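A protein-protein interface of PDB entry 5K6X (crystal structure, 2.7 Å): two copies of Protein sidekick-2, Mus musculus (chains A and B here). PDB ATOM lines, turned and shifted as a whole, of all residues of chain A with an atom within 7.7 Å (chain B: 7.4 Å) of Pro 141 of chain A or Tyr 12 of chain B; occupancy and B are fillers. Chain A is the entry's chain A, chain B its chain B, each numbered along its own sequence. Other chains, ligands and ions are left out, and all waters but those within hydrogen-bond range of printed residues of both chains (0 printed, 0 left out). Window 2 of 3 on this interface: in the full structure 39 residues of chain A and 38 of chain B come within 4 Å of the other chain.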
ATOM      1  N   VAL A 130       5.539  -5.381  35.075  1.00  0.00           N
ATOM      2  CA  VAL A 130       5.698  -4.434  36.173  1.00  0.00           C
ATOM      3  C   VAL A 130       4.906  -3.150  35.973  1.00  0.00           C
ATOM      4  O   VAL A 130       5.004  -2.501  34.935  1.00  0.00           O
ATOM      5  CB  VAL A 130       7.185  -4.080  36.377  1.00  0.00           C
ATOM      6  CG1 VAL A 130       7.331  -2.826  37.214  1.00  0.00           C
ATOM      7  CG2 VAL A 130       7.914  -5.246  37.031  1.00  0.00           C
ATOM      8  N   THR A 131       4.109  -2.801  36.978  1.00  0.00           N
ATOM      9  CA  THR A 131       3.425  -1.514  37.014  1.00  0.00           C
ATOM     10  C   THR A 131       4.082  -0.605  38.052  1.00  0.00           C
ATOM     11  O   THR A 131       4.232  -0.984  39.214  1.00  0.00           O
ATOM     12  CB  THR A 131       1.927  -1.677  37.344  1.00  0.00           C
ATOM     13  OG1 THR A 131       1.280  -2.400  36.289  1.00  0.00           O
ATOM     14  CG2 THR A 131       1.260  -0.317  37.503  1.00  0.00           C
ATOM     15  N   LYS A 138      -0.902   4.899  39.729  1.00  0.00           N
ATOM     16  CA  LYS A 138      -0.279   4.214  38.599  1.00  0.00           C
ATOM     17  C   LYS A 138       0.422   5.191  37.663  1.00  0.00           C
ATOM     18  O   LYS A 138      -0.066   6.294  37.423  1.00  0.00           O
ATOM     19  CB  LYS A 138      -1.312   3.405  37.810  1.00  0.00           C
ATOM     20  CG  LYS A 138      -1.963   2.274  38.584  1.00  0.00           C
ATOM     21  CD  LYS A 138      -2.836   1.429  37.671  1.00  0.00           C
ATOM     22  CE  LYS A 138      -3.564   0.340  38.442  1.00  0.00           C
ATOM     23  NZ  LYS A 138      -4.860  -0.025  37.804  1.00  0.00           N
ATOM     24  N   ILE A 139       1.574   4.780  37.143  1.00  0.00           N
ATOM     25  CA  ILE A 139       2.321   5.603  36.205  1.00  0.00           C
ATOM     26  C   ILE A 139       2.377   4.945  34.832  1.00  0.00           C
ATOM     27  O   ILE A 139       3.296   4.177  34.544  1.00  0.00           O
ATOM     28  CB  ILE A 139       3.762   5.861  36.685  1.00  0.00           C
ATOM     29  CG1 ILE A 139       3.780   6.287  38.150  1.00  0.00           C
ATOM     30  CG2 ILE A 139       4.433   6.914  35.820  1.00  0.00           C
ATOM     31  CD1 ILE A 139       5.175   6.476  38.690  1.00  0.00           C
ATOM     32  N   PRO A 140       1.387   5.235  33.978  1.00  0.00           N
ATOM     33  CA  PRO A 140       1.423   4.720  32.606  1.00  0.00           C
ATOM     34  C   PRO A 140       2.480   5.453  31.792  1.00  0.00           C
ATOM     35  O   PRO A 140       2.820   6.584  32.138  1.00  0.00           O
ATOM     36  CB  PRO A 140       0.017   5.016  32.083  1.00  0.00           C
ATOM     37  CG  PRO A 140      -0.418   6.210  32.861  1.00  0.00           C
ATOM     38  CD  PRO A 140       0.179   6.037  34.236  1.00  0.00           C
ATOM     39  N   PRO A 141       2.999   4.818  30.731  1.00  0.00           N
ATOM     40  CA  PRO A 141       3.977   5.488  29.867  1.00  0.00           C
ATOM     41  C   PRO A 141       3.400   6.749  29.225  1.00  0.00           C
ATOM     42  O   PRO A 141       2.190   6.834  29.013  1.00  0.00           O
ATOM     43  CB  PRO A 141       4.295   4.429  28.806  1.00  0.00           C
ATOM     44  CG  PRO A 141       3.954   3.129  29.455  1.00  0.00           C
ATOM     45  CD  PRO A 141       2.774   3.420  30.330  1.00  0.00           C
ATOM     46  N   SER A 142       4.264   7.708  28.912  1.00  0.00           N
ATOM     47  CA  SER A 142       3.830   8.948  28.282  1.00  0.00           C
ATOM     48  C   SER A 142       4.976   9.594  27.517  1.00  0.00           C
ATOM     49  O   SER A 142       6.026   8.982  27.320  1.00  0.00           O
ATOM     50  CB  SER A 142       3.275   9.920  29.325  1.00  0.00           C
ATOM     51  OG  SER A 142       4.313  10.467  30.118  1.00  0.00           O
ATOM     52  N   SER A 143       4.769  10.835  27.089  1.00  0.00           N
ATOM     53  CA  SER A 143       5.778  11.564  26.330  1.00  0.00           C
ATOM     54  C   SER A 143       7.037  11.822  27.155  1.00  0.00           C
ATOM     55  O   SER A 143       8.133  11.926  26.606  1.00  0.00           O
ATOM     56  CB  SER A 143       5.206  12.888  25.825  1.00  0.00           C
ATOM     57  OG  SER A 143       3.909  12.708  25.284  1.00  0.00           O
ATOM     58  N   ARG A 144       6.878  11.925  28.471  1.00  0.00           N
ATOM     59  CA  ARG A 144       8.011  12.182  29.353  1.00  0.00           C
ATOM     60  C   ARG A 144       8.296  11.004  30.280  1.00  0.00           C
ATOM     61  O   ARG A 144       9.309  10.987  30.981  1.00  0.00           O
ATOM     62  CB  ARG A 144       7.764  13.450  30.175  1.00  0.00           C
ATOM     63  CG  ARG A 144       6.500  13.408  31.014  1.00  0.00           C
ATOM     64  CD  ARG A 144       6.250  14.741  31.694  1.00  0.00           C
ATOM     65  NE  ARG A 144       7.148  14.966  32.821  1.00  0.00           N
ATOM     66  CZ  ARG A 144       6.885  14.603  34.072  1.00  0.00           C
ATOM     67  NH1 ARG A 144       5.745  13.997  34.370  1.00  0.00           N
ATOM     68  NH2 ARG A 144       7.764  14.849  35.031  1.00  0.00           N
ATOM     69  N   ILE A 145       7.405  10.018  30.277  1.00  0.00           N
ATOM     70  CA  ILE A 145       7.581   8.830  31.104  1.00  0.00           C
ATOM     71  C   ILE A 145       7.770   7.578  30.256  1.00  0.00           C
ATOM     72  O   ILE A 145       6.864   7.163  29.538  1.00  0.00           O
ATOM     73  CB  ILE A 145       6.382   8.613  32.045  1.00  0.00           C
ATOM     74  CG1 ILE A 145       6.072   9.896  32.822  1.00  0.00           C
ATOM     75  CG2 ILE A 145       6.661   7.465  33.001  1.00  0.00           C
ATOM     76  CD1 ILE A 145       7.107  10.241  33.867  1.00  0.00           C
ATOM     77  N   ALA A 146       8.955   6.982  30.349  1.00  0.00           N
ATOM     78  CA  ALA A 146       9.250   5.742  29.641  1.00  0.00           C
ATOM     79  C   ALA A 146       9.459   4.588  30.615  1.00  0.00           C
ATOM     80  O   ALA A 146      10.062   4.759  31.675  1.00  0.00           O
ATOM     81  CB  ALA A 146      10.474   5.911  28.755  1.00  0.00           C
ATOM     82  N   ILE A 147       8.953   3.415  30.249  1.00  0.00           N
ATOM     83  CA  ILE A 147       9.179   2.203  31.026  1.00  0.00           C
ATOM     84  C   ILE A 147       9.798   1.139  30.128  1.00  0.00           C
ATOM     85  O   ILE A 147       9.185   0.697  29.155  1.00  0.00           O
ATOM     86  CB  ILE A 147       7.877   1.673  31.653  1.00  0.00           C
ATOM     87  CG1 ILE A 147       7.163   2.787  32.420  1.00  0.00           C
ATOM     88  CG2 ILE A 147       8.174   0.501  32.574  1.00  0.00           C
ATOM     89  CD1 ILE A 147       5.733   2.460  32.791  1.00  0.00           C
ATOM     90  N   THR A 148      11.018   0.731  30.459  1.00  0.00           N
ATOM     91  CA  THR A 148      11.808  -0.121  29.576  1.00  0.00           C
ATOM     92  C   THR A 148      11.428  -1.597  29.657  1.00  0.00           C
ATOM     93  O   THR A 148      10.631  -2.005  30.503  1.00  0.00           O
ATOM     94  CB  THR A 148      13.310   0.008  29.882  1.00  0.00           C
ATOM     95  OG1 THR A 148      13.587  -0.544  31.175  1.00  0.00           O
ATOM     96  CG2 THR A 148      13.738   1.469  29.851  1.00  0.00           C
ATOM     97  N   LEU A 153      12.050   2.522  35.223  1.00  0.00           N
ATOM     98  CA  LEU A 153      11.259   3.737  35.068  1.00  0.00           C
ATOM     99  C   LEU A 153      12.152   4.925  34.725  1.00  0.00           C
ATOM    100  O   LEU A 153      13.119   5.208  35.433  1.00  0.00           O
ATOM    101  CB  LEU A 153      10.467   4.025  36.344  1.00  0.00           C
ATOM    102  CG  LEU A 153       9.611   5.293  36.376  1.00  0.00           C
ATOM    103  CD1 LEU A 153       8.450   5.185  35.402  1.00  0.00           C
ATOM    104  CD2 LEU A 153       9.106   5.550  37.782  1.00  0.00           C
ATOM    105  N   ASP A 249       4.949   2.397  21.503  1.00  0.00           N
ATOM    106  CA  ASP A 249       5.363   2.933  22.799  1.00  0.00           C
ATOM    107  C   ASP A 249       6.098   4.258  22.635  1.00  0.00           C
ATOM    108  O   ASP A 249       7.232   4.406  23.090  1.00  0.00           O
ATOM    109  CB  ASP A 249       6.239   1.927  23.547  1.00  0.00           C
ATOM    110  CG  ASP A 249       6.325   2.217  25.033  1.00  0.00           C
ATOM    111  OD1 ASP A 249       5.523   3.038  25.528  1.00  0.00           O
ATOM    112  OD2 ASP A 249       7.194   1.625  25.707  1.00  0.00           O
ATOM    113  N   TYR A 250       5.436   5.214  21.984  1.00  0.00           N
ATOM    114  CA  TYR A 250       6.023   6.517  21.676  1.00  0.00           C
ATOM    115  C   TYR A 250       7.322   6.346  20.898  1.00  0.00           C
ATOM    116  O   TYR A 250       8.324   7.000  21.186  1.00  0.00           O
ATOM    117  CB  TYR A 250       6.251   7.329  22.954  1.00  0.00           C
ATOM    118  CG  TYR A 250       4.990   7.537  23.762  1.00  0.00           C
ATOM    119  CD1 TYR A 250       4.165   8.630  23.527  1.00  0.00           C
ATOM    120  CD2 TYR A 250       4.609   6.628  24.741  1.00  0.00           C
ATOM    121  CE1 TYR A 250       3.006   8.821  24.255  1.00  0.00           C
ATOM    122  CE2 TYR A 250       3.452   6.810  25.475  1.00  0.00           C
ATOM    123  CZ  TYR A 250       2.655   7.908  25.225  1.00  0.00           C
ATOM    124  OH  TYR A 250       1.503   8.092  25.954  1.00  0.00           O
ATOM    125  N   ARG A 252       9.484   4.114  20.966  1.00  0.00           N
ATOM    126  CA  ARG A 252      10.614   3.646  21.764  1.00  0.00           C
ATOM    127  C   ARG A 252      10.822   2.140  21.603  1.00  0.00           C
ATOM    128  O   ARG A 252      11.890   1.617  21.915  1.00  0.00           O
ATOM    129  CB  ARG A 252      10.413   4.003  23.238  1.00  0.00           C
ATOM    130  CG  ARG A 252      10.312   5.497  23.493  1.00  0.00           C
ATOM    131  CD  ARG A 252      10.418   5.829  24.974  1.00  0.00           C
ATOM    132  NE  ARG A 252       9.106   5.917  25.609  1.00  0.00           N
ATOM    133  CZ  ARG A 252       8.514   7.058  25.951  1.00  0.00           C
ATOM    134  NH1 ARG A 252       9.116   8.218  25.718  1.00  0.00           N
ATOM    135  NH2 ARG A 252       7.318   7.039  26.524  1.00  0.00           N
ATOM    136  N   ARG A 253       9.796   1.448  21.118  1.00  0.00           N
ATOM    137  CA  ARG A 253       9.876   0.007  20.904  1.00  0.00           C
ATOM    138  C   ARG A 253       9.823  -0.344  19.424  1.00  0.00           C
ATOM    139  O   ARG A 253       8.973   0.155  18.687  1.00  0.00           O
ATOM    140  CB  ARG A 253       8.742  -0.715  21.636  1.00  0.00           C
ATOM    141  CG  ARG A 253       8.701  -0.485  23.134  1.00  0.00           C
ATOM    142  CD  ARG A 253       9.621  -1.424  23.883  1.00  0.00           C
ATOM    143  NE  ARG A 253       9.502  -1.252  25.329  1.00  0.00           N
ATOM    144  CZ  ARG A 253       8.512  -1.750  26.064  1.00  0.00           C
ATOM    145  NH1 ARG A 253       7.545  -2.454  25.493  1.00  0.00           N
ATOM    146  NH2 ARG A 253       8.489  -1.545  27.374  1.00  0.00           N
ATOM    147  N   VAL B   9      -7.247   6.698  31.682  1.00  0.00           N
ATOM    148  CA  VAL B   9      -6.348   5.878  30.882  1.00  0.00           C
ATOM    149  C   VAL B   9      -7.099   4.681  30.320  1.00  0.00           C
ATOM    150  O   VAL B   9      -7.539   3.812  31.074  1.00  0.00           O
ATOM    151  CB  VAL B   9      -5.140   5.391  31.699  1.00  0.00           C
ATOM    152  CG1 VAL B   9      -4.160   4.642  30.805  1.00  0.00           C
ATOM    153  CG2 VAL B   9      -4.458   6.563  32.389  1.00  0.00           C
ATOM    154  N   PRO B  10      -7.256   4.640  28.989  1.00  0.00           N
ATOM    155  CA  PRO B  10      -7.971   3.552  28.316  1.00  0.00           C
ATOM    156  C   PRO B  10      -7.264   2.221  28.530  1.00  0.00           C
ATOM    157  O   PRO B  10      -6.043   2.204  28.689  1.00  0.00           O
ATOM    158  CB  PRO B  10      -7.940   3.961  26.838  1.00  0.00           C
ATOM    159  CG  PRO B  10      -7.647   5.425  26.844  1.00  0.00           C
ATOM    160  CD  PRO B  10      -6.776   5.655  28.037  1.00  0.00           C
ATOM    161  N   PRO B  11      -8.023   1.116  28.554  1.00  0.00           N
ATOM    162  CA  PRO B  11      -7.403  -0.195  28.767  1.00  0.00           C
ATOM    163  C   PRO B  11      -6.391  -0.524  27.677  1.00  0.00           C
ATOM    164  O   PRO B  11      -6.555  -0.106  26.532  1.00  0.00           O
ATOM    165  CB  PRO B  11      -8.593  -1.164  28.720  1.00  0.00           C
ATOM    166  CG  PRO B  11      -9.793  -0.319  29.003  1.00  0.00           C
ATOM    167  CD  PRO B  11      -9.487   1.027  28.425  1.00  0.00           C
ATOM    168  N   TYR B  12      -5.343  -1.250  28.049  1.00  0.00           N
ATOM    169  CA  TYR B  12      -4.364  -1.743  27.090  1.00  0.00           C
ATOM    170  C   TYR B  12      -3.642  -2.940  27.692  1.00  0.00           C
ATOM    171  O   TYR B  12      -3.521  -3.048  28.913  1.00  0.00           O
ATOM    172  CB  TYR B  12      -3.365  -0.650  26.696  1.00  0.00           C
ATOM    173  CG  TYR B  12      -2.415  -0.236  27.798  1.00  0.00           C
ATOM    174  CD1 TYR B  12      -1.148  -0.802  27.898  1.00  0.00           C
ATOM    175  CD2 TYR B  12      -2.774   0.733  28.728  1.00  0.00           C
ATOM    176  CE1 TYR B  12      -0.274  -0.424  28.899  1.00  0.00           C
ATOM    177  CE2 TYR B  12      -1.904   1.117  29.731  1.00  0.00           C
ATOM    178  CZ  TYR B  12      -0.656   0.537  29.811  1.00  0.00           C
ATOM    179  OH  TYR B  12       0.213   0.916  30.809  1.00  0.00           O
ATOM    180  N   PHE B  13      -3.161  -3.834  26.837  1.00  0.00           N
ATOM    181  CA  PHE B  13      -2.491  -5.037  27.308  1.00  0.00           C
ATOM    182  C   PHE B  13      -0.992  -4.815  27.470  1.00  0.00           C
ATOM    183  O   PHE B  13      -0.345  -4.228  26.606  1.00  0.00           O
ATOM    184  CB  PHE B  13      -2.759  -6.200  26.355  1.00  0.00           C
ATOM    185  CG  PHE B  13      -4.177  -6.685  26.385  1.00  0.00           C
ATOM    186  CD1 PHE B  13      -5.063  -6.339  25.379  1.00  0.00           C
ATOM    187  CD2 PHE B  13      -4.631  -7.472  27.430  1.00  0.00           C
ATOM    188  CE1 PHE B  13      -6.373  -6.780  25.407  1.00  0.00           C
ATOM    189  CE2 PHE B  13      -5.940  -7.917  27.462  1.00  0.00           C
ATOM    190  CZ  PHE B  13      -6.811  -7.568  26.451  1.00  0.00           C
ATOM    191  N   LYS B  14      -0.450  -5.277  28.591  1.00  0.00           N
ATOM    192  CA  LYS B  14       0.984  -5.203  28.836  1.00  0.00           C
ATOM    193  C   LYS B  14       1.696  -6.352  28.129  1.00  0.00           C
ATOM    194  O   LYS B  14       2.857  -6.231  27.744  1.00  0.00           O
ATOM    195  CB  LYS B  14       1.275  -5.235  30.338  1.00  0.00           C
ATOM    196  CG  LYS B  14       0.772  -4.013  31.090  1.00  0.00           C
ATOM    197  CD  LYS B  14       1.716  -3.621  32.217  1.00  0.00           C
ATOM    198  CE  LYS B  14       1.779  -4.697  33.287  1.00  0.00           C
ATOM    199  NZ  LYS B  14       0.444  -4.971  33.889  1.00  0.00           N
ATOM    200  N   THR B  15       0.988  -7.465  27.961  1.00  0.00           N
ATOM    201  CA  THR B  15       1.505  -8.598  27.199  1.00  0.00           C
ATOM    202  C   THR B  15       0.371  -9.493  26.706  1.00  0.00           C
ATOM    203  O   THR B  15      -0.774  -9.359  27.139  1.00  0.00           O
ATOM    204  CB  THR B  15       2.493  -9.445  28.029  1.00  0.00           C
ATOM    205  OG1 THR B  15       3.208 -10.333  27.160  1.00  0.00           O
ATOM    206  CG2 THR B  15       1.756 -10.260  29.076  1.00  0.00           C
ATOM    207  N   CYS B  33      -5.000 -12.100  32.596  1.00  0.00           N
ATOM    208  CA  CYS B  33      -5.293 -10.980  31.714  1.00  0.00           C
ATOM    209  C   CYS B  33      -4.391  -9.813  32.083  1.00  0.00           C
ATOM    210  O   CYS B  33      -4.735  -8.997  32.938  1.00  0.00           O
ATOM    211  CB  CYS B  33      -6.762 -10.573  31.812  1.00  0.00           C
ATOM    212  SG  CYS B  33      -7.259  -9.312  30.618  1.00  0.00           S
ATOM    213  N   MET B  34      -3.234  -9.741  31.435  1.00  0.00           N
ATOM    214  CA  MET B  34      -2.244  -8.724  31.761  1.00  0.00           C
ATOM    215  C   MET B  34      -2.577  -7.406  31.077  1.00  0.00           C
ATOM    216  O   MET B  34      -1.980  -7.053  30.059  1.00  0.00           O
ATOM    217  CB  MET B  34      -0.844  -9.190  31.359  1.00  0.00           C
ATOM    218  CG  MET B  34      -0.469 -10.552  31.921  1.00  0.00           C
ATOM    219  SD  MET B  34      -0.601 -10.632  33.714  1.00  0.00           S
ATOM    220  CE  MET B  34       0.594  -9.389  34.189  1.00  0.00           C
ATOM    221  N   ALA B  35      -3.543  -6.687  31.640  1.00  0.00           N
ATOM    222  CA  ALA B  35      -3.965  -5.409  31.087  1.00  0.00           C
ATOM    223  C   ALA B  35      -3.762  -4.274  32.083  1.00  0.00           C
ATOM    224  O   ALA B  35      -3.802  -4.479  33.296  1.00  0.00           O
ATOM    225  CB  ALA B  35      -5.421  -5.475  30.655  1.00  0.00           C
ATOM    226  N   GLU B  36      -3.539  -3.075  31.560  1.00  0.00           N
ATOM    227  CA  GLU B  36      -3.451  -1.888  32.393  1.00  0.00           C
ATOM    228  C   GLU B  36      -4.472  -0.857  31.942  1.00  0.00           C
ATOM    229  O   GLU B  36      -4.979  -0.922  30.823  1.00  0.00           O
ATOM    230  CB  GLU B  36      -2.040  -1.297  32.359  1.00  0.00           C
ATOM    231  CG  GLU B  36      -1.180  -1.698  33.545  1.00  0.00           C
ATOM    232  CD  GLU B  36      -1.783  -1.270  34.872  1.00  0.00           C
ATOM    233  OE1 GLU B  36      -1.539  -1.961  35.884  1.00  0.00           O
ATOM    234  OE2 GLU B  36      -2.498  -0.245  34.904  1.00  0.00           O
ATOM    235  N   GLY B  37      -4.770   0.096  32.819  1.00  0.00           N
ATOM    236  CA  GLY B  37      -5.739   1.129  32.515  1.00  0.00           C
ATOM    237  C   GLY B  37      -6.323   1.743  33.769  1.00  0.00           C
ATOM    238  O   GLY B  37      -5.989   1.339  34.883  1.00  0.00           O
ATOM    239  N   SER B  38      -7.198   2.726  33.585  1.00  0.00           N
ATOM    240  CA  SER B  38      -7.792   3.448  34.702  1.00  0.00           C
ATOM    241  C   SER B  38      -8.738   2.592  35.536  1.00  0.00           C
ATOM    242  O   SER B  38      -9.258   1.578  35.071  1.00  0.00           O
ATOM    243  CB  SER B  38      -8.539   4.682  34.194  1.00  0.00           C
ATOM    244  OG  SER B  38      -7.632   5.690  33.792  1.00  0.00           O
ATOM    245  N   LEU B  41     -10.565  -1.240  36.781  1.00  0.00           N
ATOM    246  CA  LEU B  41     -10.172  -2.175  35.735  1.00  0.00           C
ATOM    247  C   LEU B  41     -10.710  -3.567  36.057  1.00  0.00           C
ATOM    248  O   LEU B  41     -10.198  -4.252  36.944  1.00  0.00           O
ATOM    249  CB  LEU B  41      -8.649  -2.205  35.586  1.00  0.00           C
ATOM    250  CG  LEU B  41      -8.095  -2.700  34.251  1.00  0.00           C
ATOM    251  CD1 LEU B  41      -8.472  -1.730  33.140  1.00  0.00           C
ATOM    252  CD2 LEU B  41      -6.589  -2.885  34.322  1.00  0.00           C
ATOM    253  N   VAL B  78     -11.156  -7.097  29.210  1.00  0.00           N
ATOM    254  CA  VAL B  78     -10.822  -6.088  30.204  1.00  0.00           C
ATOM    255  C   VAL B  78     -11.582  -4.806  29.894  1.00  0.00           C
ATOM    256  O   VAL B  78     -11.729  -4.429  28.732  1.00  0.00           O
ATOM    257  CB  VAL B  78      -9.298  -5.825  30.253  1.00  0.00           C
ATOM    258  CG1 VAL B  78      -8.775  -5.370  28.898  1.00  0.00           C
ATOM    259  CG2 VAL B  78      -8.959  -4.817  31.333  1.00  0.00           C
ATOM    260  N   ASN B  80     -12.915  -0.651  31.589  1.00  0.00           N
ATOM    261  CA  ASN B  80     -13.094   0.375  32.605  1.00  0.00           C
ATOM    262  C   ASN B  80     -14.095   1.406  32.095  1.00  0.00           C
ATOM    263  O   ASN B  80     -14.927   1.093  31.243  1.00  0.00           O
ATOM    264  CB  ASN B  80     -11.758   1.020  32.992  1.00  0.00           C
ATOM    265  CG  ASN B  80     -11.016   1.618  31.807  1.00  0.00           C
ATOM    266  OD1 ASN B  80     -11.598   1.898  30.760  1.00  0.00           O
ATOM    267  ND2 ASN B  80      -9.713   1.815  31.973  1.00  0.00           N
ATOM    268  N   LEU B  85     -11.619  -4.168  25.885  1.00  0.00           N
ATOM    269  CA  LEU B  85     -10.774  -4.818  24.887  1.00  0.00           C
ATOM    270  C   LEU B  85     -10.925  -6.332  24.914  1.00  0.00           C
ATOM    271  O   LEU B  85     -11.040  -6.934  25.980  1.00  0.00           O
ATOM    272  CB  LEU B  85      -9.303  -4.457  25.098  1.00  0.00           C
ATOM    273  CG  LEU B  85      -8.899  -2.990  24.967  1.00  0.00           C
ATOM    274  CD1 LEU B  85      -7.413  -2.845  25.236  1.00  0.00           C
ATOM    275  CD2 LEU B  85      -9.258  -2.452  23.592  1.00  0.00           C
ATOM    276  N   MET B 362     -13.437   2.107  22.970  1.00  0.00           N
ATOM    277  CA  MET B 362     -12.320   1.347  22.425  1.00  0.00           C
ATOM    278  C   MET B 362     -12.693   0.648  21.124  1.00  0.00           C
ATOM    279  O   MET B 362     -13.645  -0.128  21.077  1.00  0.00           O
ATOM    280  CB  MET B 362     -11.824   0.315  23.442  1.00  0.00           C
ATOM    281  CG  MET B 362     -11.355   0.911  24.757  1.00  0.00           C
ATOM    282  SD  MET B 362     -10.126   2.209  24.532  1.00  0.00           S
ATOM    283  CE  MET B 362      -8.757   1.280  23.848  1.00  0.00           C
ATOM    284  N   GLN B 375      -3.920  -8.353  17.355  1.00  0.00           N
ATOM    285  CA  GLN B 375      -4.863  -7.278  17.635  1.00  0.00           C
ATOM    286  C   GLN B 375      -4.171  -5.944  17.878  1.00  0.00           C
ATOM    287  O   GLN B 375      -3.051  -5.886  18.384  1.00  0.00           O
ATOM    288  CB  GLN B 375      -5.739  -7.640  18.844  1.00  0.00           C
ATOM    289  CG  GLN B 375      -4.984  -7.811  20.161  1.00  0.00           C
ATOM    290  CD  GLN B 375      -4.787  -6.506  20.912  1.00  0.00           C
ATOM    291  OE1 GLN B 375      -5.566  -5.565  20.761  1.00  0.00           O
ATOM    292  NE2 GLN B 375      -3.738  -6.441  21.721  1.00  0.00           N
ATOM    293  N   SER B 377      -5.445  -1.771  19.092  1.00  0.00           N
ATOM    294  CA  SER B 377      -6.575  -1.025  19.622  1.00  0.00           C
ATOM    295  C   SER B 377      -6.358   0.479  19.558  1.00  0.00           C
ATOM    296  O   SER B 377      -5.270   0.954  19.228  1.00  0.00           O
ATOM    297  CB  SER B 377      -6.854  -1.446  21.067  1.00  0.00           C
ATOM    298  OG  SER B 377      -5.735  -1.192  21.900  1.00  0.00           O
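OE1 of Glu 36 of chain B lies within hydrogen-bond range of OG1 of Thr 131 of chain A (2.9 Å).
O of Gly 37 of chain B is in hydrogen-bond range of NZ of Lys 138 of chain A, 3.4 Å away.
NZ of Lys 138 of chain A is in salt-bridge range of OE2 of Glu 36 of chain B, 3.7 Å away.
The backbone carbonyl oxygen (O) of Tyr 12 of chain B lies within hydrogen-bond range of the backbone NH (N) of Glu 36 of chain B.
O of Pro 141 of chain A sits at hydrogen-bond distance from OH of Tyr 250 of chain A, at 3.4 Å.
The backbone NH of Lys 14 of chain B lies within hydrogen-bond range of the backbone carbonyl oxygen of Met 34 of chain B, at 2.8 Å.
Among the printed residues, merely in contact across the chains: Pro 141 of chain A with Tyr 12 of chain B and Thr 131 of chain A with Lys 14 of chain B.
Pro 141 of chain A touches one residue of chain B.
Tyr 12 of chain B touches one residue of chain A.
Printed residues of chain A within 4 Å of Glu 36 of chain B: Thr 131 (2.9 Å) and Lys 138 (3.3 Å).
Printed residues of chain A within 4 Å of Lys 14 of chain B: Thr 131 (3.6 Å).
The nearest residue of chain B that does not touch Pro 141 of chain A is Val 9 of chain B (7.0 Å).
The nearest printed residue of chain A that does not touch Glu 36 of chain B is Val 130 of chain A (6.4 Å).
Among the printed residues, 5 pairs touch across the chains.
Among the printed residues, Asp or Glu carboxylates within 4 Å of a Lys or Arg side-chain nitrogen of the other chain: Lys 138 of chain A with Glu 36 of chain B (3.7 Å).
No position is printed for both chains.
Of the 5 pairs that touch across the chains among the printed residues, none has its exchanged pair printed and touching as well.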
